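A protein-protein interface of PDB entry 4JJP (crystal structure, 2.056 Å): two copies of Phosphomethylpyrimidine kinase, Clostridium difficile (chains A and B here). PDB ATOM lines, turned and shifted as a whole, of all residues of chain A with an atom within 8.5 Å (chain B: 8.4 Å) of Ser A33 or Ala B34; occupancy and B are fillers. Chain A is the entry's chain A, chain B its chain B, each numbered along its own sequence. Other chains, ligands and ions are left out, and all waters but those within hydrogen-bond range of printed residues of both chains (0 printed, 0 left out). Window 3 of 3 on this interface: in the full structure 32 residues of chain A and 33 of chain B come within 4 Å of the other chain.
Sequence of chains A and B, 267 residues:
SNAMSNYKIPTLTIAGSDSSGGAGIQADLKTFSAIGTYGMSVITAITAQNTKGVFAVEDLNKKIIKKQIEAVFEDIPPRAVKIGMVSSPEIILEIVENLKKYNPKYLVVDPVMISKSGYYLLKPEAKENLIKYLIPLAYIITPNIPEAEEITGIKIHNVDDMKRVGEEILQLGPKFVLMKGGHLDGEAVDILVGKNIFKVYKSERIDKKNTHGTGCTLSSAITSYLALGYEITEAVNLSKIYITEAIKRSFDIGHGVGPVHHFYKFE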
ATOM      1  N   ILE A   9      -7.085  23.074 -17.823  1.00  0.00           N
ATOM      2  CA  ILE A   9      -6.539  22.150 -16.829  1.00  0.00           C
ATOM      3  C   ILE A   9      -6.362  20.776 -17.498  1.00  0.00           C
ATOM      4  O   ILE A   9      -7.344  20.126 -17.803  1.00  0.00           O
ATOM      5  CB  ILE A   9      -7.523  22.020 -15.637  1.00  0.00           C
ATOM      6  CG1 ILE A   9      -7.901  23.406 -15.107  1.00  0.00           C
ATOM      7  CG2 ILE A   9      -6.925  21.133 -14.546  1.00  0.00           C
ATOM      8  CD1 ILE A   9      -6.700  24.227 -14.636  1.00  0.00           C
ATOM      9  N   THR A  11      -5.854  16.846 -18.251  1.00  0.00           N
ATOM     10  CA  THR A  11      -6.105  15.540 -17.659  1.00  0.00           C
ATOM     11  C   THR A  11      -5.721  14.486 -18.687  1.00  0.00           C
ATOM     12  O   THR A  11      -6.021  14.631 -19.863  1.00  0.00           O
ATOM     13  CB  THR A  11      -7.567  15.359 -17.263  1.00  0.00           C
ATOM     14  OG1 THR A  11      -8.385  15.854 -18.312  1.00  0.00           O
ATOM     15  CG2 THR A  11      -7.904  16.138 -16.007  1.00  0.00           C
ATOM     16  N   GLN A  26     -11.905   7.261 -25.927  1.00  0.00           N
ATOM     17  CA  GLN A  26     -12.976   8.042 -26.529  1.00  0.00           C
ATOM     18  C   GLN A  26     -13.979   8.473 -25.455  1.00  0.00           C
ATOM     19  O   GLN A  26     -14.317   9.625 -25.371  1.00  0.00           O
ATOM     20  CB  GLN A  26     -13.667   7.269 -27.671  1.00  0.00           C
ATOM     21  CG  GLN A  26     -12.825   7.095 -28.957  1.00  0.00           C
ATOM     22  CD  GLN A  26     -11.701   6.075 -28.884  1.00  0.00           C
ATOM     23  OE1 GLN A  26     -11.575   5.300 -27.927  1.00  0.00           O
ATOM     24  NE2 GLN A  26     -10.888   6.049 -29.928  1.00  0.00           N
ATOM     25  N   ALA A  27     -14.421   7.535 -24.617  1.00  0.00           N
ATOM     26  CA  ALA A  27     -15.369   7.840 -23.543  1.00  0.00           C
ATOM     27  C   ALA A  27     -14.726   8.808 -22.559  1.00  0.00           C
ATOM     28  O   ALA A  27     -15.372   9.761 -22.132  1.00  0.00           O
ATOM     29  CB  ALA A  27     -15.798   6.580 -22.819  1.00  0.00           C
ATOM     30  N   ASP A  28     -13.456   8.561 -22.212  1.00  0.00           N
ATOM     31  CA  ASP A  28     -12.724   9.428 -21.299  1.00  0.00           C
ATOM     32  C   ASP A  28     -12.598  10.855 -21.845  1.00  0.00           C
ATOM     33  O   ASP A  28     -12.832  11.814 -21.118  1.00  0.00           O
ATOM     34  CB  ASP A  28     -11.320   8.887 -21.009  1.00  0.00           C
ATOM     35  CG  ASP A  28     -11.325   7.547 -20.267  1.00  0.00           C
ATOM     36  OD1 ASP A  28     -12.356   7.129 -19.688  1.00  0.00           O
ATOM     37  OD2 ASP A  28     -10.271   6.899 -20.248  1.00  0.00           O
ATOM     38  N   LEU A  29     -12.239  10.992 -23.121  1.00  0.00           N
ATOM     39  CA  LEU A  29     -12.072  12.310 -23.709  1.00  0.00           C
ATOM     40  C   LEU A  29     -13.376  13.069 -23.780  1.00  0.00           C
ATOM     41  O   LEU A  29     -13.374  14.284 -23.628  1.00  0.00           O
ATOM     42  CB  LEU A  29     -11.386  12.253 -25.072  1.00  0.00           C
ATOM     43  CG  LEU A  29      -9.928  11.785 -25.071  1.00  0.00           C
ATOM     44  CD1 LEU A  29      -9.517  11.587 -26.545  1.00  0.00           C
ATOM     45  CD2 LEU A  29      -9.010  12.797 -24.350  1.00  0.00           C
ATOM     46  N   LYS A  30     -14.483  12.359 -23.994  1.00  0.00           N
ATOM     47  CA  LYS A  30     -15.800  12.983 -24.013  1.00  0.00           C
ATOM     48  C   LYS A  30     -16.133  13.561 -22.631  1.00  0.00           C
ATOM     49  O   LYS A  30     -16.605  14.693 -22.520  1.00  0.00           O
ATOM     50  CB  LYS A  30     -16.856  11.956 -24.420  1.00  0.00           C
ATOM     51  CG  LYS A  30     -16.683  11.435 -25.818  1.00  0.00           C
ATOM     52  CD  LYS A  30     -17.670  10.327 -26.161  1.00  0.00           C
ATOM     53  CE  LYS A  30     -17.352   9.701 -27.523  1.00  0.00           C
ATOM     54  NZ  LYS A  30     -18.466   8.827 -28.008  1.00  0.00           N
ATOM     55  N   THR A  31     -15.878  12.776 -21.583  1.00  0.00           N
ATOM     56  CA  THR A  31     -16.146  13.206 -20.195  1.00  0.00           C
ATOM     57  C   THR A  31     -15.252  14.399 -19.833  1.00  0.00           C
ATOM     58  O   THR A  31     -15.734  15.435 -19.375  1.00  0.00           O
ATOM     59  CB  THR A  31     -15.926  12.057 -19.173  1.00  0.00           C
ATOM     60  OG1 THR A  31     -16.781  10.954 -19.498  1.00  0.00           O
ATOM     61  CG2 THR A  31     -16.197  12.505 -17.720  1.00  0.00           C
ATOM     62  N   PHE A  32     -13.949  14.243 -20.054  1.00  0.00           N
ATOM     63  CA  PHE A  32     -13.017  15.345 -19.804  1.00  0.00           C
ATOM     64  C   PHE A  32     -13.550  16.662 -20.412  1.00  0.00           C
ATOM     65  O   PHE A  32     -13.677  17.679 -19.739  1.00  0.00           O
ATOM     66  CB  PHE A  32     -11.636  15.069 -20.403  1.00  0.00           C
ATOM     67  CG  PHE A  32     -10.874  13.961 -19.748  1.00  0.00           C
ATOM     68  CD1 PHE A  32     -11.162  13.526 -18.460  1.00  0.00           C
ATOM     69  CD2 PHE A  32      -9.766  13.416 -20.391  1.00  0.00           C
ATOM     70  CE1 PHE A  32     -10.409  12.530 -17.881  1.00  0.00           C
ATOM     71  CE2 PHE A  32      -9.002  12.423 -19.787  1.00  0.00           C
ATOM     72  CZ  PHE A  32      -9.314  11.998 -18.547  1.00  0.00           C
ATOM     73  N   SER A  33     -13.860  16.604 -21.696  1.00  0.00           N
ATOM     74  CA  SER A  33     -14.340  17.755 -22.448  1.00  0.00           C
ATOM     75  C   SER A  33     -15.639  18.343 -21.898  1.00  0.00           C
ATOM     76  O   SER A  33     -15.777  19.566 -21.799  1.00  0.00           O
ATOM     77  CB  SER A  33     -14.490  17.380 -23.932  1.00  0.00           C
ATOM     78  OG  SER A  33     -15.139  18.404 -24.670  1.00  0.00           O
ATOM     79  N   ALA A  34     -16.587  17.485 -21.528  1.00  0.00           N
ATOM     80  CA  ALA A  34     -17.871  17.953 -20.995  1.00  0.00           C
ATOM     81  C   ALA A  34     -17.695  18.626 -19.639  1.00  0.00           C
ATOM     82  O   ALA A  34     -18.362  19.606 -19.343  1.00  0.00           O
ATOM     83  CB  ALA A  34     -18.889  16.792 -20.899  1.00  0.00           C
ATOM     84  N   ILE A  35     -16.784  18.106 -18.824  1.00  0.00           N
ATOM     85  CA  ILE A  35     -16.564  18.659 -17.487  1.00  0.00           C
ATOM     86  C   ILE A  35     -15.741  19.940 -17.536  1.00  0.00           C
ATOM     87  O   ILE A  35     -15.949  20.822 -16.724  1.00  0.00           O
ATOM     88  CB  ILE A  35     -15.940  17.607 -16.540  1.00  0.00           C
ATOM     89  CG1 ILE A  35     -16.984  16.496 -16.269  1.00  0.00           C
ATOM     90  CG2 ILE A  35     -15.471  18.249 -15.229  1.00  0.00           C
ATOM     91  CD1 ILE A  35     -16.490  15.315 -15.497  1.00  0.00           C
ATOM     92  N   GLY A  36     -14.809  20.049 -18.469  1.00  0.00           N
ATOM     93  CA  GLY A  36     -14.021  21.271 -18.593  1.00  0.00           C
ATOM     94  C   GLY A  36     -12.511  21.174 -18.484  1.00  0.00           C
ATOM     95  O   GLY A  36     -11.858  22.197 -18.385  1.00  0.00           O
ATOM     96  N   THR A  37     -11.956  19.967 -18.508  1.00  0.00           N
ATOM     97  CA  THR A  37     -10.505  19.776 -18.467  1.00  0.00           C
ATOM     98  C   THR A  37      -9.974  19.543 -19.896  1.00  0.00           C
ATOM     99  O   THR A  37     -10.742  19.197 -20.784  1.00  0.00           O
ATOM    100  CB  THR A  37     -10.139  18.640 -17.501  1.00  0.00           C
ATOM    101  OG1 THR A  37     -10.795  17.439 -17.902  1.00  0.00           O
ATOM    102  CG2 THR A  37     -10.601  19.014 -16.056  1.00  0.00           C
ATOM    103  N   TYR A  38      -8.676  19.744 -20.108  1.00  0.00           N
ATOM    104  CA  TYR A  38      -8.054  19.614 -21.412  1.00  0.00           C
ATOM    105  C   TYR A  38      -7.565  18.187 -21.559  1.00  0.00           C
ATOM    106  O   TYR A  38      -6.578  17.787 -20.934  1.00  0.00           O
ATOM    107  CB  TYR A  38      -6.901  20.614 -21.551  1.00  0.00           C
ATOM    108  CG  TYR A  38      -6.169  20.525 -22.869  1.00  0.00           C
ATOM    109  CD1 TYR A  38      -6.576  21.260 -23.970  1.00  0.00           C
ATOM    110  CD2 TYR A  38      -5.064  19.699 -23.008  1.00  0.00           C
ATOM    111  CE1 TYR A  38      -5.900  21.175 -25.186  1.00  0.00           C
ATOM    112  CE2 TYR A  38      -4.388  19.600 -24.206  1.00  0.00           C
ATOM    113  CZ  TYR A  38      -4.811  20.338 -25.292  1.00  0.00           C
ATOM    114  OH  TYR A  38      -4.119  20.230 -26.469  1.00  0.00           O
ATOM    115  N   GLY A  39      -8.263  17.419 -22.391  1.00  0.00           N
ATOM    116  CA  GLY A  39      -7.982  16.011 -22.561  1.00  0.00           C
ATOM    117  C   GLY A  39      -6.741  15.669 -23.359  1.00  0.00           C
ATOM    118  O   GLY A  39      -6.481  16.262 -24.392  1.00  0.00           O
ATOM    119  N   MET A  40      -5.985  14.700 -22.848  1.00  0.00           N
ATOM    120  CA  MET A  40      -4.794  14.137 -23.481  1.00  0.00           C
ATOM    121  C   MET A  40      -4.905  12.611 -23.346  1.00  0.00           C
ATOM    122  O   MET A  40      -5.610  12.119 -22.460  1.00  0.00           O
ATOM    123  CB  MET A  40      -3.543  14.583 -22.747  1.00  0.00           C
ATOM    124  CG  MET A  40      -3.365  16.099 -22.703  1.00  0.00           C
ATOM    125  SD  MET A  40      -1.796  16.567 -21.975  1.00  0.00           S
ATOM    126  CE  MET A  40      -2.014  16.228 -20.262  1.00  0.00           C
ATOM    127  N   SER A 220     -13.390   8.621 -15.150  1.00  0.00           N
ATOM    128  CA  SER A 220     -12.922   9.771 -15.916  1.00  0.00           C
ATOM    129  C   SER A 220     -13.457  11.089 -15.304  1.00  0.00           C
ATOM    130  O   SER A 220     -12.712  12.079 -15.214  1.00  0.00           O
ATOM    131  CB  SER A 220     -13.235   9.613 -17.419  1.00  0.00           C
ATOM    132  OG  SER A 220     -14.619   9.608 -17.701  1.00  0.00           O
ATOM    133  N   SER A 224     -11.312  14.342 -13.715  1.00  0.00           N
ATOM    134  CA  SER A 224     -11.521  15.741 -14.072  1.00  0.00           C
ATOM    135  C   SER A 224     -11.747  16.615 -12.850  1.00  0.00           C
ATOM    136  O   SER A 224     -11.181  17.704 -12.752  1.00  0.00           O
ATOM    137  CB  SER A 224     -12.726  15.930 -15.006  1.00  0.00           C
ATOM    138  OG  SER A 224     -12.464  15.432 -16.293  1.00  0.00           O
ATOM    139  N   TYR A 242     -22.859  14.650 -12.330  1.00  0.00           N
ATOM    140  CA  TYR A 242     -22.573  14.703 -13.752  1.00  0.00           C
ATOM    141  C   TYR A 242     -23.274  13.547 -14.468  1.00  0.00           C
ATOM    142  O   TYR A 242     -24.014  13.763 -15.425  1.00  0.00           O
ATOM    143  CB  TYR A 242     -21.069  14.641 -14.025  1.00  0.00           C
ATOM    144  CG  TYR A 242     -20.785  14.476 -15.495  1.00  0.00           C
ATOM    145  CD1 TYR A 242     -21.004  15.532 -16.393  1.00  0.00           C
ATOM    146  CD2 TYR A 242     -20.328  13.261 -16.004  1.00  0.00           C
ATOM    147  CE1 TYR A 242     -20.762  15.369 -17.763  1.00  0.00           C
ATOM    148  CE2 TYR A 242     -20.090  13.098 -17.364  1.00  0.00           C
ATOM    149  CZ  TYR A 242     -20.299  14.145 -18.234  1.00  0.00           C
ATOM    150  OH  TYR A 242     -20.048  13.955 -19.576  1.00  0.00           O
ATOM    151  N   GLN B  26      -8.041  13.280 -31.149  1.00  0.00           N
ATOM    152  CA  GLN B  26      -8.308  13.807 -29.793  1.00  0.00           C
ATOM    153  C   GLN B  26      -9.008  15.144 -29.858  1.00  0.00           C
ATOM    154  O   GLN B  26     -10.019  15.353 -29.204  1.00  0.00           O
ATOM    155  CB  GLN B  26      -7.020  13.975 -28.969  1.00  0.00           C
ATOM    156  CG  GLN B  26      -6.393  12.701 -28.467  1.00  0.00           C
ATOM    157  CD  GLN B  26      -5.685  11.882 -29.507  1.00  0.00           C
ATOM    158  OE1 GLN B  26      -5.508  12.294 -30.648  1.00  0.00           O
ATOM    159  NE2 GLN B  26      -5.255  10.700 -29.107  1.00  0.00           N
ATOM    160  N   ALA B  27      -8.453  16.053 -30.637  1.00  0.00           N
ATOM    161  CA  ALA B  27      -9.042  17.396 -30.812  1.00  0.00           C
ATOM    162  C   ALA B  27     -10.417  17.294 -31.419  1.00  0.00           C
ATOM    163  O   ALA B  27     -11.322  18.008 -31.024  1.00  0.00           O
ATOM    164  CB  ALA B  27      -8.142  18.282 -31.670  1.00  0.00           C
ATOM    165  N   ASP B  28     -10.576  16.406 -32.401  1.00  0.00           N
ATOM    166  CA  ASP B  28     -11.881  16.209 -33.059  1.00  0.00           C
ATOM    167  C   ASP B  28     -12.941  15.673 -32.096  1.00  0.00           C
ATOM    168  O   ASP B  28     -14.057  16.217 -32.006  1.00  0.00           O
ATOM    169  CB  ASP B  28     -11.740  15.269 -34.259  1.00  0.00           C
ATOM    170  CG  ASP B  28     -10.831  15.830 -35.352  1.00  0.00           C
ATOM    171  OD1 ASP B  28     -10.572  17.059 -35.381  1.00  0.00           O
ATOM    172  OD2 ASP B  28     -10.384  15.028 -36.201  1.00  0.00           O
ATOM    173  N   LEU B  29     -12.599  14.627 -31.348  1.00  0.00           N
ATOM    174  CA  LEU B  29     -13.540  14.035 -30.390  1.00  0.00           C
ATOM    175  C   LEU B  29     -13.962  15.026 -29.306  1.00  0.00           C
ATOM    176  O   LEU B  29     -15.126  15.039 -28.899  1.00  0.00           O
ATOM    177  CB  LEU B  29     -12.942  12.776 -29.738  1.00  0.00           C
ATOM    178  CG  LEU B  29     -12.730  11.550 -30.633  1.00  0.00           C
ATOM    179  CD1 LEU B  29     -11.937  10.452 -29.917  1.00  0.00           C
ATOM    180  CD2 LEU B  29     -14.088  11.034 -31.147  1.00  0.00           C
ATOM    181  N   LYS B  30     -13.014  15.845 -28.844  1.00  0.00           N
ATOM    182  CA  LYS B  30     -13.287  16.863 -27.828  1.00  0.00           C
ATOM    183  C   LYS B  30     -14.285  17.848 -28.341  1.00  0.00           C
ATOM    184  O   LYS B  30     -15.164  18.264 -27.595  1.00  0.00           O
ATOM    185  CB  LYS B  30     -12.042  17.648 -27.482  1.00  0.00           C
ATOM    186  CG  LYS B  30     -10.976  16.853 -26.732  1.00  0.00           C
ATOM    187  CD  LYS B  30      -9.728  17.714 -26.740  1.00  0.00           C
ATOM    188  CE  LYS B  30      -8.622  17.150 -25.967  1.00  0.00           C
ATOM    189  NZ  LYS B  30      -7.537  18.124 -26.003  1.00  0.00           N
ATOM    190  N   THR B  31     -14.116  18.236 -29.605  1.00  0.00           N
ATOM    191  CA  THR B  31     -15.019  19.163 -30.275  1.00  0.00           C
ATOM    192  C   THR B  31     -16.401  18.566 -30.499  1.00  0.00           C
ATOM    193  O   THR B  31     -17.421  19.226 -30.251  1.00  0.00           O
ATOM    194  CB  THR B  31     -14.453  19.597 -31.636  1.00  0.00           C
ATOM    195  OG1 THR B  31     -13.186  20.225 -31.436  1.00  0.00           O
ATOM    196  CG2 THR B  31     -15.399  20.578 -32.356  1.00  0.00           C
ATOM    197  N   PHE B  32     -16.455  17.329 -30.988  1.00  0.00           N
ATOM    198  CA  PHE B  32     -17.747  16.690 -31.202  1.00  0.00           C
ATOM    199  C   PHE B  32     -18.493  16.697 -29.857  1.00  0.00           C
ATOM    200  O   PHE B  32     -19.667  17.077 -29.785  1.00  0.00           O
ATOM    201  CB  PHE B  32     -17.632  15.251 -31.691  1.00  0.00           C
ATOM    202  CG  PHE B  32     -16.947  15.064 -33.038  1.00  0.00           C
ATOM    203  CD1 PHE B  32     -17.037  16.004 -34.053  1.00  0.00           C
ATOM    204  CD2 PHE B  32     -16.305  13.865 -33.308  1.00  0.00           C
ATOM    205  CE1 PHE B  32     -16.424  15.798 -35.299  1.00  0.00           C
ATOM    206  CE2 PHE B  32     -15.704  13.629 -34.548  1.00  0.00           C
ATOM    207  CZ  PHE B  32     -15.770  14.602 -35.553  1.00  0.00           C
ATOM    208  N   SER B  33     -17.793  16.264 -28.807  1.00  0.00           N
ATOM    209  CA  SER B  33     -18.341  16.213 -27.456  1.00  0.00           C
ATOM    210  C   SER B  33     -18.852  17.594 -27.055  1.00  0.00           C
ATOM    211  O   SER B  33     -20.021  17.749 -26.702  1.00  0.00           O
ATOM    212  CB  SER B  33     -17.285  15.678 -26.466  1.00  0.00           C
ATOM    213  OG  SER B  33     -17.785  15.563 -25.140  1.00  0.00           O
ATOM    214  N   ALA B  34     -18.021  18.622 -27.137  1.00  0.00           N
ATOM    215  CA  ALA B  34     -18.517  19.974 -26.771  1.00  0.00           C
ATOM    216  C   ALA B  34     -19.711  20.452 -27.591  1.00  0.00           C
ATOM    217  O   ALA B  34     -20.625  21.095 -27.050  1.00  0.00           O
ATOM    218  CB  ALA B  34     -17.388  21.011 -26.840  1.00  0.00           C
ATOM    219  N   ILE B  35     -19.755  20.150 -28.882  1.00  0.00           N
ATOM    220  CA  ILE B  35     -20.860  20.665 -29.719  1.00  0.00           C
ATOM    221  C   ILE B  35     -22.145  19.856 -29.544  1.00  0.00           C
ATOM    222  O   ILE B  35     -23.253  20.392 -29.677  1.00  0.00           O
ATOM    223  CB  ILE B  35     -20.472  20.783 -31.199  1.00  0.00           C
ATOM    224  CG1 ILE B  35     -19.338  21.792 -31.339  1.00  0.00           C
ATOM    225  CG2 ILE B  35     -21.659  21.257 -32.038  1.00  0.00           C
ATOM    226  CD1 ILE B  35     -18.734  21.882 -32.728  1.00  0.00           C
ATOM    227  N   GLY B  36     -21.992  18.568 -29.260  1.00  0.00           N
ATOM    228  CA  GLY B  36     -23.130  17.691 -28.999  1.00  0.00           C
ATOM    229  C   GLY B  36     -23.437  16.604 -30.011  1.00  0.00           C
ATOM    230  O   GLY B  36     -24.608  16.271 -30.208  1.00  0.00           O
ATOM    231  N   THR B  37     -22.409  16.061 -30.665  1.00  0.00           N
ATOM    232  CA  THR B  37     -22.597  14.934 -31.572  1.00  0.00           C
ATOM    233  C   THR B  37     -21.884  13.753 -30.918  1.00  0.00           C
ATOM    234  O   THR B  37     -21.094  13.959 -30.008  1.00  0.00           O
ATOM    235  CB  THR B  37     -22.102  15.222 -32.984  1.00  0.00           C
ATOM    236  OG1 THR B  37     -20.703  15.512 -32.957  1.00  0.00           O
ATOM    237  CG2 THR B  37     -22.883  16.403 -33.575  1.00  0.00           C
ATOM    238  N   THR B 217      -9.862  22.017 -34.867  1.00  0.00           N
ATOM    239  CA  THR B 217     -11.093  22.296 -34.187  1.00  0.00           C
ATOM    240  C   THR B 217     -12.130  22.846 -35.185  1.00  0.00           C
ATOM    241  O   THR B 217     -13.299  22.441 -35.159  1.00  0.00           O
ATOM    242  CB  THR B 217     -10.843  23.255 -33.014  1.00  0.00           C
ATOM    243  OG1 THR B 217      -9.904  22.654 -32.112  1.00  0.00           O
ATOM    244  CG2 THR B 217     -12.142  23.571 -32.259  1.00  0.00           C
ATOM    245  N   SER B 224     -19.560  18.540 -37.134  1.00  0.00           N
ATOM    246  CA  SER B 224     -20.646  18.413 -36.169  1.00  0.00           C
ATOM    247  C   SER B 224     -21.875  19.198 -36.604  1.00  0.00           C
ATOM    248  O   SER B 224     -22.980  18.642 -36.639  1.00  0.00           O
ATOM    249  CB  SER B 224     -20.232  18.866 -34.763  1.00  0.00           C
ATOM    250  OG  SER B 224     -19.405  17.914 -34.132  1.00  0.00           O
ATOM    251  N   TYR B 225     -21.710  20.481 -36.921  1.00  0.00           N
ATOM    252  CA  TYR B 225     -22.879  21.268 -37.343  1.00  0.00           C
ATOM    253  C   TYR B 225     -23.541  20.782 -38.639  1.00  0.00           C
ATOM    254  O   TYR B 225     -24.771  20.913 -38.784  1.00  0.00           O
ATOM    255  CB  TYR B 225     -22.577  22.771 -37.408  1.00  0.00           C
ATOM    256  CG  TYR B 225     -22.331  23.366 -36.045  1.00  0.00           C
ATOM    257  CD1 TYR B 225     -23.358  23.455 -35.121  1.00  0.00           C
ATOM    258  CD2 TYR B 225     -21.080  23.856 -35.689  1.00  0.00           C
ATOM    259  CE1 TYR B 225     -23.147  23.990 -33.864  1.00  0.00           C
ATOM    260  CE2 TYR B 225     -20.854  24.406 -34.439  1.00  0.00           C
ATOM    261  CZ  TYR B 225     -21.893  24.459 -33.530  1.00  0.00           C
ATOM    262  OH  TYR B 225     -21.691  24.993 -32.295  1.00  0.00           O
ATOM    263  N   LEU B 228     -25.637  17.976 -37.559  1.00  0.00           N
ATOM    264  CA  LEU B 228     -26.819  18.475 -36.825  1.00  0.00           C
ATOM    265  C   LEU B 228     -27.889  19.111 -37.724  1.00  0.00           C
ATOM    266  O   LEU B 228     -28.957  19.512 -37.238  1.00  0.00           O
ATOM    267  CB  LEU B 228     -26.384  19.465 -35.742  1.00  0.00           C
ATOM    268  CG  LEU B 228     -25.701  18.793 -34.550  1.00  0.00           C
ATOM    269  CD1 LEU B 228     -25.139  19.824 -33.608  1.00  0.00           C
ATOM    270  CD2 LEU B 228     -26.705  17.900 -33.831  1.00  0.00           C
ATOM    271  N   TYR B 242     -17.791  29.003 -31.969  1.00  0.00           N
ATOM    272  CA  TYR B 242     -17.358  27.919 -31.061  1.00  0.00           C
ATOM    273  C   TYR B 242     -15.885  28.041 -30.686  1.00  0.00           C
ATOM    274  O   TYR B 242     -15.520  27.909 -29.519  1.00  0.00           O
ATOM    275  CB  TYR B 242     -17.609  26.516 -31.654  1.00  0.00           C
ATOM    276  CG  TYR B 242     -16.959  25.438 -30.817  1.00  0.00           C
ATOM    277  CD1 TYR B 242     -17.576  24.970 -29.661  1.00  0.00           C
ATOM    278  CD2 TYR B 242     -15.705  24.920 -31.151  1.00  0.00           C
ATOM    279  CE1 TYR B 242     -16.976  23.991 -28.864  1.00  0.00           C
ATOM    280  CE2 TYR B 242     -15.097  23.953 -30.354  1.00  0.00           C
ATOM    281  CZ  TYR B 242     -15.742  23.493 -29.213  1.00  0.00           C
ATOM    282  OH  TYR B 242     -15.161  22.531 -28.417  1.00  0.00           O
ATOM    283  N   GLU B 245     -14.874  30.808 -27.899  1.00  0.00           N
ATOM    284  CA  GLU B 245     -15.021  30.335 -26.523  1.00  0.00           C
ATOM    285  C   GLU B 245     -13.888  29.377 -26.090  1.00  0.00           C
ATOM    286  O   GLU B 245     -13.549  29.312 -24.901  1.00  0.00           O
ATOM    287  CB  GLU B 245     -16.371  29.642 -26.346  1.00  0.00           C
ATOM    288  CG  GLU B 245     -17.581  30.484 -26.746  1.00  0.00           C
ATOM    289  CD  GLU B 245     -18.878  29.720 -26.576  1.00  0.00           C
ATOM    290  OE1 GLU B 245     -19.118  29.184 -25.467  1.00  0.00           O
ATOM    291  OE2 GLU B 245     -19.662  29.665 -27.548  1.00  0.00           O
ATOM    292  N   ALA B 246     -13.314  28.644 -27.046  1.00  0.00           N
ATOM    293  CA  ALA B 246     -12.219  27.713 -26.777  1.00  0.00           C
ATOM    294  C   ALA B 246     -10.869  28.319 -27.172  1.00  0.00           C
ATOM    295  O   ALA B 246     -10.517  29.426 -26.756  1.00  0.00           O
ATOM    296  CB  ALA B 246     -12.456  26.415 -27.533  1.00  0.00           C
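The side-chain amino group of Lys B30 lies within hydrogen-bond range of the backbone carbonyl oxygen of Gly A39, 2.7 Å away. The backbone carbonyl oxygen (O) of Lys A30 lies within hydrogen-bond range of the side-chain hydroxyl (OG) of Ser B33 (3.0 Å). The backbone carbonyl oxygen of Lys B30 lies within hydrogen-bond range of the side-chain hydroxyl of Ser A33 (2.9 Å).
The backbone carbonyl oxygen (O) of Ile A9 is in hydrogen-bond range of the backbone NH (N) of Tyr A38 (2.7 Å). O of Tyr A38 lies within hydrogen-bond range of N of Thr A11, at 2.9 Å.
Leu B29 touches Gln A26. Gln B26 touches Leu A29. Ser A33 touches Ser B33. Ser A33 touches Ala B34 (OG to N, 3.8 Å). NZ of Lys B30 touches CE1 of Tyr A38, 3.6 Å away.
Thr A11 touches none of the printed residues of chain B. Of the printed residues of chain B, Leu A29 touches Gln B26 (3.8 Å). Printed residues of chain B within 4 Å of Lys A30: Ser B33. Ser A33 touches just these residues of chain B: Lys B30 (2.9 Å), Ser B33 (3.9 Å) and Ala B34 (3.8 Å). Printed residues of chain B within 4 Å of Tyr A38: Lys B30 (3.6 Å). Printed residues of chain A within 4 Å of Ser B33: Lys A30 and Ser A33. The nearest residue of chain B that does not touch Ser A33 is Thr B31 (5.0 Å). The nearest residue of chain A that does not touch Ala B34 is Ala A34 (5.9 Å).
Printed residues of chain A that touch a printed residue of chain B: Gln A26, Leu A29, Lys A30, Ser A33, Tyr A38 and Gly A39. Hydrophobic or aromatic side chains of chain A that line the printed part of chain B: Leu A29 and Tyr A38. Hydrophobic or aromatic side chains of chain B that line the printed part of chain A: Leu B29. Among the printed residues, 8 pairs touch across the chains. Among the printed residues, no Asp or Glu carboxylate lies within 4 Å of a Lys or Arg side-chain nitrogen of the other chain.
Gln A26 touches Leu B29, and with the chains exchanged Leu A29 touches Gln B26. Lys A30 touches Ser B33, and with the chains exchanged Ser A33 touches Lys B30. Ser A33 touches its own counterpart, Ser B33. Ser A33 touches Ala B34, but with the chains exchanged Ala A34 does not touch Ser B33 (4.3 Å). Positions printed for both chains: 26, 27, 28, 29, 30, 31, 32, 33, 34, 35, 36, 37, 224 and 242.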
